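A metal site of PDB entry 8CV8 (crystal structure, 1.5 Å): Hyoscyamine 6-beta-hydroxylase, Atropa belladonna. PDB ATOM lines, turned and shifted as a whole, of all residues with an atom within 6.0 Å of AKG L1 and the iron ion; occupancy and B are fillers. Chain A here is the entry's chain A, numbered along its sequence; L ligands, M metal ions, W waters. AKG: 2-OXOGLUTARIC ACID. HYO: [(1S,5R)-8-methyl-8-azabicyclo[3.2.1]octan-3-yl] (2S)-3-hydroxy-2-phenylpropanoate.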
ATOM      1  N   LYS A 129      16.338  -4.492  -8.217  1.00  0.00           N
ATOM      2  CA  LYS A 129      17.223  -3.966  -7.148  1.00  0.00           C
ATOM      3  C   LYS A 129      17.119  -4.866  -5.913  1.00  0.00           C
ATOM      4  O   LYS A 129      15.999  -5.284  -5.561  1.00  0.00           O
ATOM      5  CB  LYS A 129      16.777  -2.536  -6.813  1.00  0.00           C
ATOM      6  CG  LYS A 129      17.393  -1.901  -5.575  1.00  0.00           C
ATOM      7  CD  LYS A 129      17.080  -0.420  -5.483  1.00  0.00           C
ATOM      8  CE  LYS A 129      15.677  -0.121  -5.007  1.00  0.00           C
ATOM      9  NZ  LYS A 129      15.513  -0.368  -3.560  1.00  0.00           N
ATOM     10  N   LEU A 198      21.761   2.800   2.734  1.00  0.00           N
ATOM     11  CA  LEU A 198      21.153   1.884   1.743  1.00  0.00           C
ATOM     12  C   LEU A 198      22.233   1.527   0.735  1.00  0.00           C
ATOM     13  O   LEU A 198      22.676   2.422  -0.003  1.00  0.00           O
ATOM     14  CB  LEU A 198      19.958   2.586   1.085  1.00  0.00           C
ATOM     15  CG  LEU A 198      18.627   2.488   1.828  1.00  0.00           C
ATOM     16  CD1 LEU A 198      18.689   3.153   3.193  1.00  0.00           C
ATOM     17  CD2 LEU A 198      17.514   3.087   0.987  1.00  0.00           C
ATOM     18  N   ASN A 200      22.717  -0.384  -2.524  1.00  0.00           N
ATOM     19  CA  ASN A 200      21.814  -0.812  -3.621  1.00  0.00           C
ATOM     20  C   ASN A 200      22.601  -1.662  -4.605  1.00  0.00           C
ATOM     21  O   ASN A 200      23.660  -1.215  -5.048  1.00  0.00           O
ATOM     22  CB  ASN A 200      21.217   0.382  -4.359  1.00  0.00           C
ATOM     23  CG  ASN A 200      20.480   1.294  -3.414  1.00  0.00           C
ATOM     24  OD1 ASN A 200      19.589   0.858  -2.691  1.00  0.00           O
ATOM     25  ND2 ASN A 200      20.869   2.563  -3.391  1.00  0.00           N
ATOM     26  N   TYR A 202      22.185  -3.557  -8.236  1.00  0.00           N
ATOM     27  CA  TYR A 202      21.452  -3.652  -9.527  1.00  0.00           C
ATOM     28  C   TYR A 202      22.116  -4.738 -10.366  1.00  0.00           C
ATOM     29  O   TYR A 202      23.129  -4.474 -11.019  1.00  0.00           O
ATOM     30  CB  TYR A 202      21.466  -2.292 -10.222  1.00  0.00           C
ATOM     31  CG  TYR A 202      20.989  -1.154  -9.359  1.00  0.00           C
ATOM     32  CD1 TYR A 202      19.638  -0.867  -9.233  1.00  0.00           C
ATOM     33  CD2 TYR A 202      21.886  -0.375  -8.656  1.00  0.00           C
ATOM     34  CE1 TYR A 202      19.198   0.184  -8.452  1.00  0.00           C
ATOM     35  CE2 TYR A 202      21.456   0.675  -7.861  1.00  0.00           C
ATOM     36  CZ  TYR A 202      20.113   0.962  -7.764  1.00  0.00           C
ATOM     37  OH  TYR A 202      19.706   2.005  -6.973  1.00  0.00           O
ATOM     38  N   SER A 214      15.377   1.634 -10.090  1.00  0.00           N
ATOM     39  CA  SER A 214      14.733   2.452  -9.042  1.00  0.00           C
ATOM     40  C   SER A 214      13.761   3.402  -9.732  1.00  0.00           C
ATOM     41  O   SER A 214      14.210   4.168 -10.602  1.00  0.00           O
ATOM     42  CB  SER A 214      15.774   3.185  -8.233  1.00  0.00           C
ATOM     43  OG  SER A 214      15.269   3.598  -6.971  1.00  0.00           O
ATOM     44  N   HIS A 217      11.657   9.162  -8.048  1.00  0.00           N
ATOM     45  CA  HIS A 217      11.284   9.537  -6.662  1.00  0.00           C
ATOM     46  C   HIS A 217      12.090  10.740  -6.212  1.00  0.00           C
ATOM     47  O   HIS A 217      13.234  10.910  -6.646  1.00  0.00           O
ATOM     48  CB  HIS A 217      11.475   8.357  -5.700  1.00  0.00           C
ATOM     49  CG  HIS A 217      12.905   7.956  -5.508  1.00  0.00           C
ATOM     50  ND1 HIS A 217      13.608   7.257  -6.468  1.00  0.00           N
ATOM     51  CD2 HIS A 217      13.768   8.172  -4.494  1.00  0.00           C
ATOM     52  CE1 HIS A 217      14.842   7.062  -6.046  1.00  0.00           C
ATOM     53  NE2 HIS A 217      14.967   7.604  -4.828  1.00  0.00           N
ATOM     54  N   TYR A 218      11.518  11.520  -5.288  1.00  0.00           N
ATOM     55  CA  TYR A 218      12.292  12.262  -4.276  1.00  0.00           C
ATOM     56  C   TYR A 218      12.709  11.282  -3.188  1.00  0.00           C
ATOM     57  O   TYR A 218      11.931  10.365  -2.862  1.00  0.00           O
ATOM     58  CB  TYR A 218      11.445  13.303  -3.543  1.00  0.00           C
ATOM     59  CG  TYR A 218      10.908  14.466  -4.336  1.00  0.00           C
ATOM     60  CD1 TYR A 218      11.688  15.581  -4.602  1.00  0.00           C
ATOM     61  CD2 TYR A 218       9.589  14.480  -4.739  1.00  0.00           C
ATOM     62  CE1 TYR A 218      11.170  16.666  -5.294  1.00  0.00           C
ATOM     63  CE2 TYR A 218       9.064  15.559  -5.434  1.00  0.00           C
ATOM     64  CZ  TYR A 218       9.861  16.659  -5.704  1.00  0.00           C
ATOM     65  OH  TYR A 218       9.333  17.723  -6.389  1.00  0.00           O
ATOM     66  N   ASP A 219      13.869  11.500  -2.575  1.00  0.00           N
ATOM     67  CA  ASP A 219      14.173  10.928  -1.245  1.00  0.00           C
ATOM     68  C   ASP A 219      13.291  11.682  -0.246  1.00  0.00           C
ATOM     69  O   ASP A 219      13.258  12.920  -0.296  1.00  0.00           O
ATOM     70  CB  ASP A 219      15.665  11.021  -0.917  1.00  0.00           C
ATOM     71  CG  ASP A 219      16.564  10.141  -1.784  1.00  0.00           C
ATOM     72  OD1 ASP A 219      16.043   9.343  -2.584  1.00  0.00           O
ATOM     73  OD2 ASP A 219      17.786  10.276  -1.663  1.00  0.00           O
ATOM     74  N   THR A 224      20.520  13.485   1.144  1.00  0.00           N
ATOM     75  CA  THR A 224      21.141  12.171   0.849  1.00  0.00           C
ATOM     76  C   THR A 224      22.490  12.417   0.182  1.00  0.00           C
ATOM     77  O   THR A 224      22.560  13.286  -0.719  1.00  0.00           O
ATOM     78  CB  THR A 224      20.248  11.320  -0.071  1.00  0.00           C
ATOM     79  OG1 THR A 224      19.007  11.106   0.607  1.00  0.00           O
ATOM     80  CG2 THR A 224      20.900  10.004  -0.420  1.00  0.00           C
ATOM     81  N   LEU A 226      25.166  10.216  -2.066  1.00  0.00           N
ATOM     82  CA  LEU A 226      25.136   8.987  -2.891  1.00  0.00           C
ATOM     83  C   LEU A 226      26.550   8.794  -3.469  1.00  0.00           C
ATOM     84  O   LEU A 226      27.084   9.729  -4.066  1.00  0.00           O
ATOM     85  CB  LEU A 226      24.057   9.152  -3.965  1.00  0.00           C
ATOM     86  CG  LEU A 226      23.827   8.013  -4.955  1.00  0.00           C
ATOM     87  CD1 LEU A 226      24.960   7.881  -5.972  1.00  0.00           C
ATOM     88  CD2 LEU A 226      23.577   6.688  -4.257  1.00  0.00           C
ATOM     89  N   GLN A 228      28.690   6.492  -6.157  1.00  0.00           N
ATOM     90  CA  GLN A 228      28.525   5.618  -7.340  1.00  0.00           C
ATOM     91  C   GLN A 228      29.829   5.582  -8.131  1.00  0.00           C
ATOM     92  O   GLN A 228      30.568   6.580  -8.094  1.00  0.00           O
ATOM     93  CB  GLN A 228      27.376   6.105  -8.221  1.00  0.00           C
ATOM     94  CG  GLN A 228      27.522   7.555  -8.680  1.00  0.00           C
ATOM     95  CD  GLN A 228      26.600   7.927  -9.816  1.00  0.00           C
ATOM     96  OE1 GLN A 228      25.826   7.111 -10.315  1.00  0.00           O
ATOM     97  NE2 GLN A 228      26.669   9.167 -10.232  1.00  0.00           N
ATOM     98  N   GLY A 232      23.919   4.965 -14.489  1.00  0.00           N
ATOM     99  CA  GLY A 232      22.571   4.425 -14.224  1.00  0.00           C
ATOM    100  C   GLY A 232      21.674   5.432 -13.547  1.00  0.00           C
ATOM    101  O   GLY A 232      20.447   5.325 -13.701  1.00  0.00           O
ATOM    102  N   LEU A 233      22.264   6.376 -12.791  1.00  0.00           N
ATOM    103  CA  LEU A 233      21.486   7.408 -12.069  1.00  0.00           C
ATOM    104  C   LEU A 233      21.052   8.481 -13.070  1.00  0.00           C
ATOM    105  O   LEU A 233      21.915   8.960 -13.843  1.00  0.00           O
ATOM    106  CB  LEU A 233      22.334   8.000 -10.949  1.00  0.00           C
ATOM    107  CG  LEU A 233      21.673   9.121 -10.141  1.00  0.00           C
ATOM    108  CD1 LEU A 233      20.434   8.631  -9.416  1.00  0.00           C
ATOM    109  CD2 LEU A 233      22.678   9.714  -9.173  1.00  0.00           C
ATOM    110  N   ASN A 255      21.647  14.739  -3.027  1.00  0.00           N
ATOM    111  CA  ASN A 255      20.211  14.806  -3.402  1.00  0.00           C
ATOM    112  C   ASN A 255      19.457  15.508  -2.271  1.00  0.00           C
ATOM    113  O   ASN A 255      19.462  14.978  -1.144  1.00  0.00           O
ATOM    114  CB  ASN A 255      19.611  13.414  -3.621  1.00  0.00           C
ATOM    115  CG  ASN A 255      19.980  12.765  -4.942  1.00  0.00           C
ATOM    116  OD1 ASN A 255      19.931  13.388  -5.988  1.00  0.00           O
ATOM    117  ND2 ASN A 255      20.305  11.482  -4.909  1.00  0.00           N
ATOM    118  N   HIS A 273      14.817  11.632  -9.046  1.00  0.00           N
ATOM    119  CA  HIS A 273      15.847  10.791  -9.707  1.00  0.00           C
ATOM    120  C   HIS A 273      15.349   9.355  -9.823  1.00  0.00           C
ATOM    121  O   HIS A 273      14.429   8.962  -9.099  1.00  0.00           O
ATOM    122  CB  HIS A 273      17.180  10.900  -8.969  1.00  0.00           C
ATOM    123  CG  HIS A 273      17.078  10.588  -7.513  1.00  0.00           C
ATOM    124  ND1 HIS A 273      16.715  11.531  -6.581  1.00  0.00           N
ATOM    125  CD2 HIS A 273      17.300   9.440  -6.824  1.00  0.00           C
ATOM    126  CE1 HIS A 273      16.713  10.974  -5.384  1.00  0.00           C
ATOM    127  NE2 HIS A 273      17.077   9.710  -5.506  1.00  0.00           N
ATOM    128  N   ARG A 274      15.979   8.609 -10.719  1.00  0.00           N
ATOM    129  CA  ARG A 274      15.671   7.180 -10.976  1.00  0.00           C
ATOM    130  C   ARG A 274      16.977   6.467 -11.338  1.00  0.00           C
ATOM    131  O   ARG A 274      17.996   7.151 -11.599  1.00  0.00           O
ATOM    132  CB  ARG A 274      14.642   7.032 -12.094  1.00  0.00           C
ATOM    133  CG  ARG A 274      15.196   7.275 -13.487  1.00  0.00           C
ATOM    134  CD  ARG A 274      14.127   7.199 -14.565  1.00  0.00           C
ATOM    135  NE  ARG A 274      14.712   7.427 -15.866  1.00  0.00           N
ATOM    136  CZ  ARG A 274      14.019   7.609 -16.993  1.00  0.00           C
ATOM    137  NH1 ARG A 274      12.698   7.591 -16.968  1.00  0.00           N
ATOM    138  NH2 ARG A 274      14.659   7.823 -18.131  1.00  0.00           N
ATOM    139  N   VAL A 275      16.935   5.153 -11.362  1.00  0.00           N
ATOM    140  CA  VAL A 275      18.087   4.310 -11.789  1.00  0.00           C
ATOM    141  C   VAL A 275      17.600   3.354 -12.868  1.00  0.00           C
ATOM    142  O   VAL A 275      16.596   2.656 -12.655  1.00  0.00           O
ATOM    143  CB  VAL A 275      18.729   3.557 -10.616  1.00  0.00           C
ATOM    144  CG1 VAL A 275      19.891   2.707 -11.102  1.00  0.00           C
ATOM    145  CG2 VAL A 275      19.176   4.521  -9.528  1.00  0.00           C
ATOM    146  N   ARG A 283      25.813  -3.150 -10.795  1.00  0.00           N
ATOM    147  CA  ARG A 283      26.123  -1.797 -10.275  1.00  0.00           C
ATOM    148  C   ARG A 283      25.804  -1.812  -8.784  1.00  0.00           C
ATOM    149  O   ARG A 283      24.759  -2.359  -8.397  1.00  0.00           O
ATOM    150  CB  ARG A 283      25.296  -0.738 -10.997  1.00  0.00           C
ATOM    151  CG  ARG A 283      25.439   0.670 -10.433  1.00  0.00           C
ATOM    152  CD  ARG A 283      24.790   1.679 -11.362  1.00  0.00           C
ATOM    153  NE  ARG A 283      24.899   3.038 -10.861  1.00  0.00           N
ATOM    154  CZ  ARG A 283      24.110   3.591  -9.946  1.00  0.00           C
ATOM    155  NH1 ARG A 283      23.119   2.901  -9.405  1.00  0.00           N
ATOM    156  NH2 ARG A 283      24.308   4.840  -9.583  1.00  0.00           N
ATOM    157  N   SER A 285      25.558   1.005  -5.573  1.00  0.00           N
ATOM    158  CA  SER A 285      25.586   2.408  -5.096  1.00  0.00           C
ATOM    159  C   SER A 285      25.393   2.403  -3.578  1.00  0.00           C
ATOM    160  O   SER A 285      24.808   1.448  -3.038  1.00  0.00           O
ATOM    161  CB  SER A 285      24.558   3.268  -5.780  1.00  0.00           C
ATOM    162  OG  SER A 285      23.250   2.926  -5.381  1.00  0.00           O
ATOM    163  N   ALA A 287      23.881   4.872  -0.706  1.00  0.00           N
ATOM    164  CA  ALA A 287      23.057   6.051  -0.385  1.00  0.00           C
ATOM    165  C   ALA A 287      23.008   6.219   1.132  1.00  0.00           C
ATOM    166  O   ALA A 287      22.588   5.274   1.814  1.00  0.00           O
ATOM    167  CB  ALA A 287      21.674   5.889  -0.961  1.00  0.00           C
ATOM    168  N   LEU A 289      21.032   8.303   3.694  1.00  0.00           N
ATOM    169  CA  LEU A 289      19.791   9.097   3.793  1.00  0.00           C
ATOM    170  C   LEU A 289      19.709   9.647   5.210  1.00  0.00           C
ATOM    171  O   LEU A 289      19.442   8.868   6.134  1.00  0.00           O
ATOM    172  CB  LEU A 289      18.594   8.209   3.471  1.00  0.00           C
ATOM    173  CG  LEU A 289      18.334   7.966   1.990  1.00  0.00           C
ATOM    174  CD1 LEU A 289      19.368   7.019   1.383  1.00  0.00           C
ATOM    175  CD2 LEU A 289      16.933   7.425   1.790  1.00  0.00           C
HETATM  176  C1  AKG L   1      18.198   5.696  -3.410  1.00  0.00           C
HETATM  177  O1  AKG L   1      17.371   6.466  -2.916  1.00  0.00           O
HETATM  178  O2  AKG L   1      18.593   4.677  -2.817  1.00  0.00           O
HETATM  179  C2  AKG L   1      18.698   5.992  -4.591  1.00  0.00           C
HETATM  180  O5  AKG L   1      18.186   6.936  -5.217  1.00  0.00           O
HETATM  181  C3  AKG L   1      19.903   5.302  -5.182  1.00  0.00           C
HETATM  182  C4  AKG L   1      20.348   5.845  -6.529  1.00  0.00           C
HETATM  183  C5  AKG L   1      21.509   5.135  -7.195  1.00  0.00           C
HETATM  184  O3  AKG L   1      22.329   5.822  -7.828  1.00  0.00           O
HETATM  185  O4  AKG L   1      21.577   3.882  -7.114  1.00  0.00           O
HETATM  186  C10 HYO L   2      13.627   3.498   0.222  1.00  0.00           C
HETATM  187  C13 HYO L   2      13.174   5.269   2.793  1.00  0.00           C
HETATM  188  C15 HYO L   2      12.495   7.194   4.158  1.00  0.00           C
HETATM  189  C17 HYO L   2      11.445   6.557   4.826  1.00  0.00           C
HETATM  190  C20 HYO L   2      11.410   9.322   4.522  1.00  0.00           C
HETATM  191  C21 HYO L   2      10.363   8.685   5.181  1.00  0.00           C
HETATM  192  C05 HYO L   2      13.155   5.556  -1.703  1.00  0.00           C
HETATM  193  C06 HYO L   2      14.562   3.972  -0.895  1.00  0.00           C
HETATM  194  C07 HYO L   2      14.327   6.368  -1.128  1.00  0.00           C
HETATM  195  C08 HYO L   2      15.256   5.292  -0.553  1.00  0.00           C
HETATM  196  C09 HYO L   2      12.053   5.263  -0.680  1.00  0.00           C
HETATM  197  C11 HYO L   2      12.552   4.535   0.554  1.00  0.00           C
HETATM  198  C12 HYO L   2      14.504   4.360  -3.318  1.00  0.00           C
HETATM  199  C14 HYO L   2      13.664   6.428   3.609  1.00  0.00           C
HETATM  200  C16 HYO L   2      14.597   5.949   4.719  1.00  0.00           C
HETATM  201  C18 HYO L   2      12.465   8.574   4.012  1.00  0.00           C
HETATM  202  C19 HYO L   2      10.380   7.306   5.322  1.00  0.00           C
HETATM  203  N04 HYO L   2      13.730   4.264  -2.065  1.00  0.00           N
HETATM  204  O01 HYO L   2      13.095   5.544   1.399  1.00  0.00           O
HETATM  205  O02 HYO L   2      12.881   4.177   3.235  1.00  0.00           O
HETATM  206  O03 HYO L   2      15.108   7.064   5.458  1.00  0.00           O
HETATM  207 FE    FE M   1      16.913   8.162  -4.028  1.00  0.00          FE
HETATM  208  O   HOH W   1      17.189   2.251  -2.560  1.00  0.00           O
HETATM  209  O   HOH W   2      17.425   2.895  -5.453  1.00  0.00           O
HETATM  210  O   HOH W   3      19.168   9.035  -3.393  1.00  0.00           O
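The side-chain hydroxyl (OH) of Tyr 202 lies within hydrogen-bond range of an oxygen (O4) of AKG L1 (2.7 Å).
The side-chain amide nitrogen of Asn 200 sits at hydrogen-bond distance from an oxygen (O2) of AKG L1 (3.2 Å).
An oxygen (O4) of AKG L1 sits at hydrogen-bond distance from the side-chain hydroxyl of Ser 285, 2.6 Å away.
The guanidinium group (NH2) of Arg 283 lies within salt-bridge range of an oxygen (O3) of AKG L1, 2.8 Å away.
The iron ion is bound by the side-chain carboxylate (OD1) of Asp 219.
O1 of AKG L1 binds the iron ion (2.1 Å).
O5 of AKG L1 is bound to the iron ion (2.1 Å).
NE2 of His 273 binds the iron ion.
The iron ion is bound by NE2 of His 217, 2.2 Å away.
The iron ion is bound by water W3.
The iron ion has six donor atoms within binding distance.
Water W3 bridges the side-chain carboxylate of Asp 219 (2.5 Å) and the side-chain amide nitrogen of Asn 255 (3.1 Å).
Water W1 lies within hydrogen-bond range of the side-chain amide oxygen (OD1) of Asn 200 (2.8 Å), an oxygen (O2) of AKG L1 (2.8 Å) and the side-chain amino group (NZ) of Lys 129 (3.3 Å).
Water W2 lies within hydrogen-bond range of OG of Ser 214, OH of Tyr 202 and O2 of AKG L1.
Leu 226 touches AKG L1 (CD1 to O3, 3.8 Å).
CD1 of Leu 233 touches O3 of AKG L1 (3.7 Å).
Val 275 touches AKG L1.
Ala 287 touches AKG L1 (CB to O2, 3.8 Å).
Hydrophobic or aromatic side chains that line AKG L1: Tyr 202, His 217, Leu 226, Leu 233, His 273, Val 275 and Ala 287.
Of the 21 residues printed, 11 come within 4 Å of AKG L1.
Within 4 Å of the iron ion: His 217, Asp 219 and His 273.
The nearest printed residue that does not touch the iron ion is Asn 255 (4.8 Å).
The guanidinium group (NH2) of Arg 283 is in hydrogen-bond range of the side-chain amide oxygen (OE1) of Gln 228, 2.8 Å away.
The side-chain hydroxyl (OG1) of Thr 224 is in hydrogen-bond range of the side-chain carboxylate (OD2) of Asp 219 (2.7 Å).
The backbone carbonyl oxygen of Ala 287 sits at hydrogen-bond distance from the backbone NH of Leu 198.
The backbone carbonyl oxygen (O) of Ser 285 is in hydrogen-bond range of the backbone NH (N) of Asn 200 (2.8 Å).
The backbone carbonyl oxygen (O) of Ser 214 is in hydrogen-bond range of the backbone NH (N) of Val 275 (3.0 Å).
N of Tyr 202 sits at hydrogen-bond distance from O of Arg 283 (2.8 Å).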
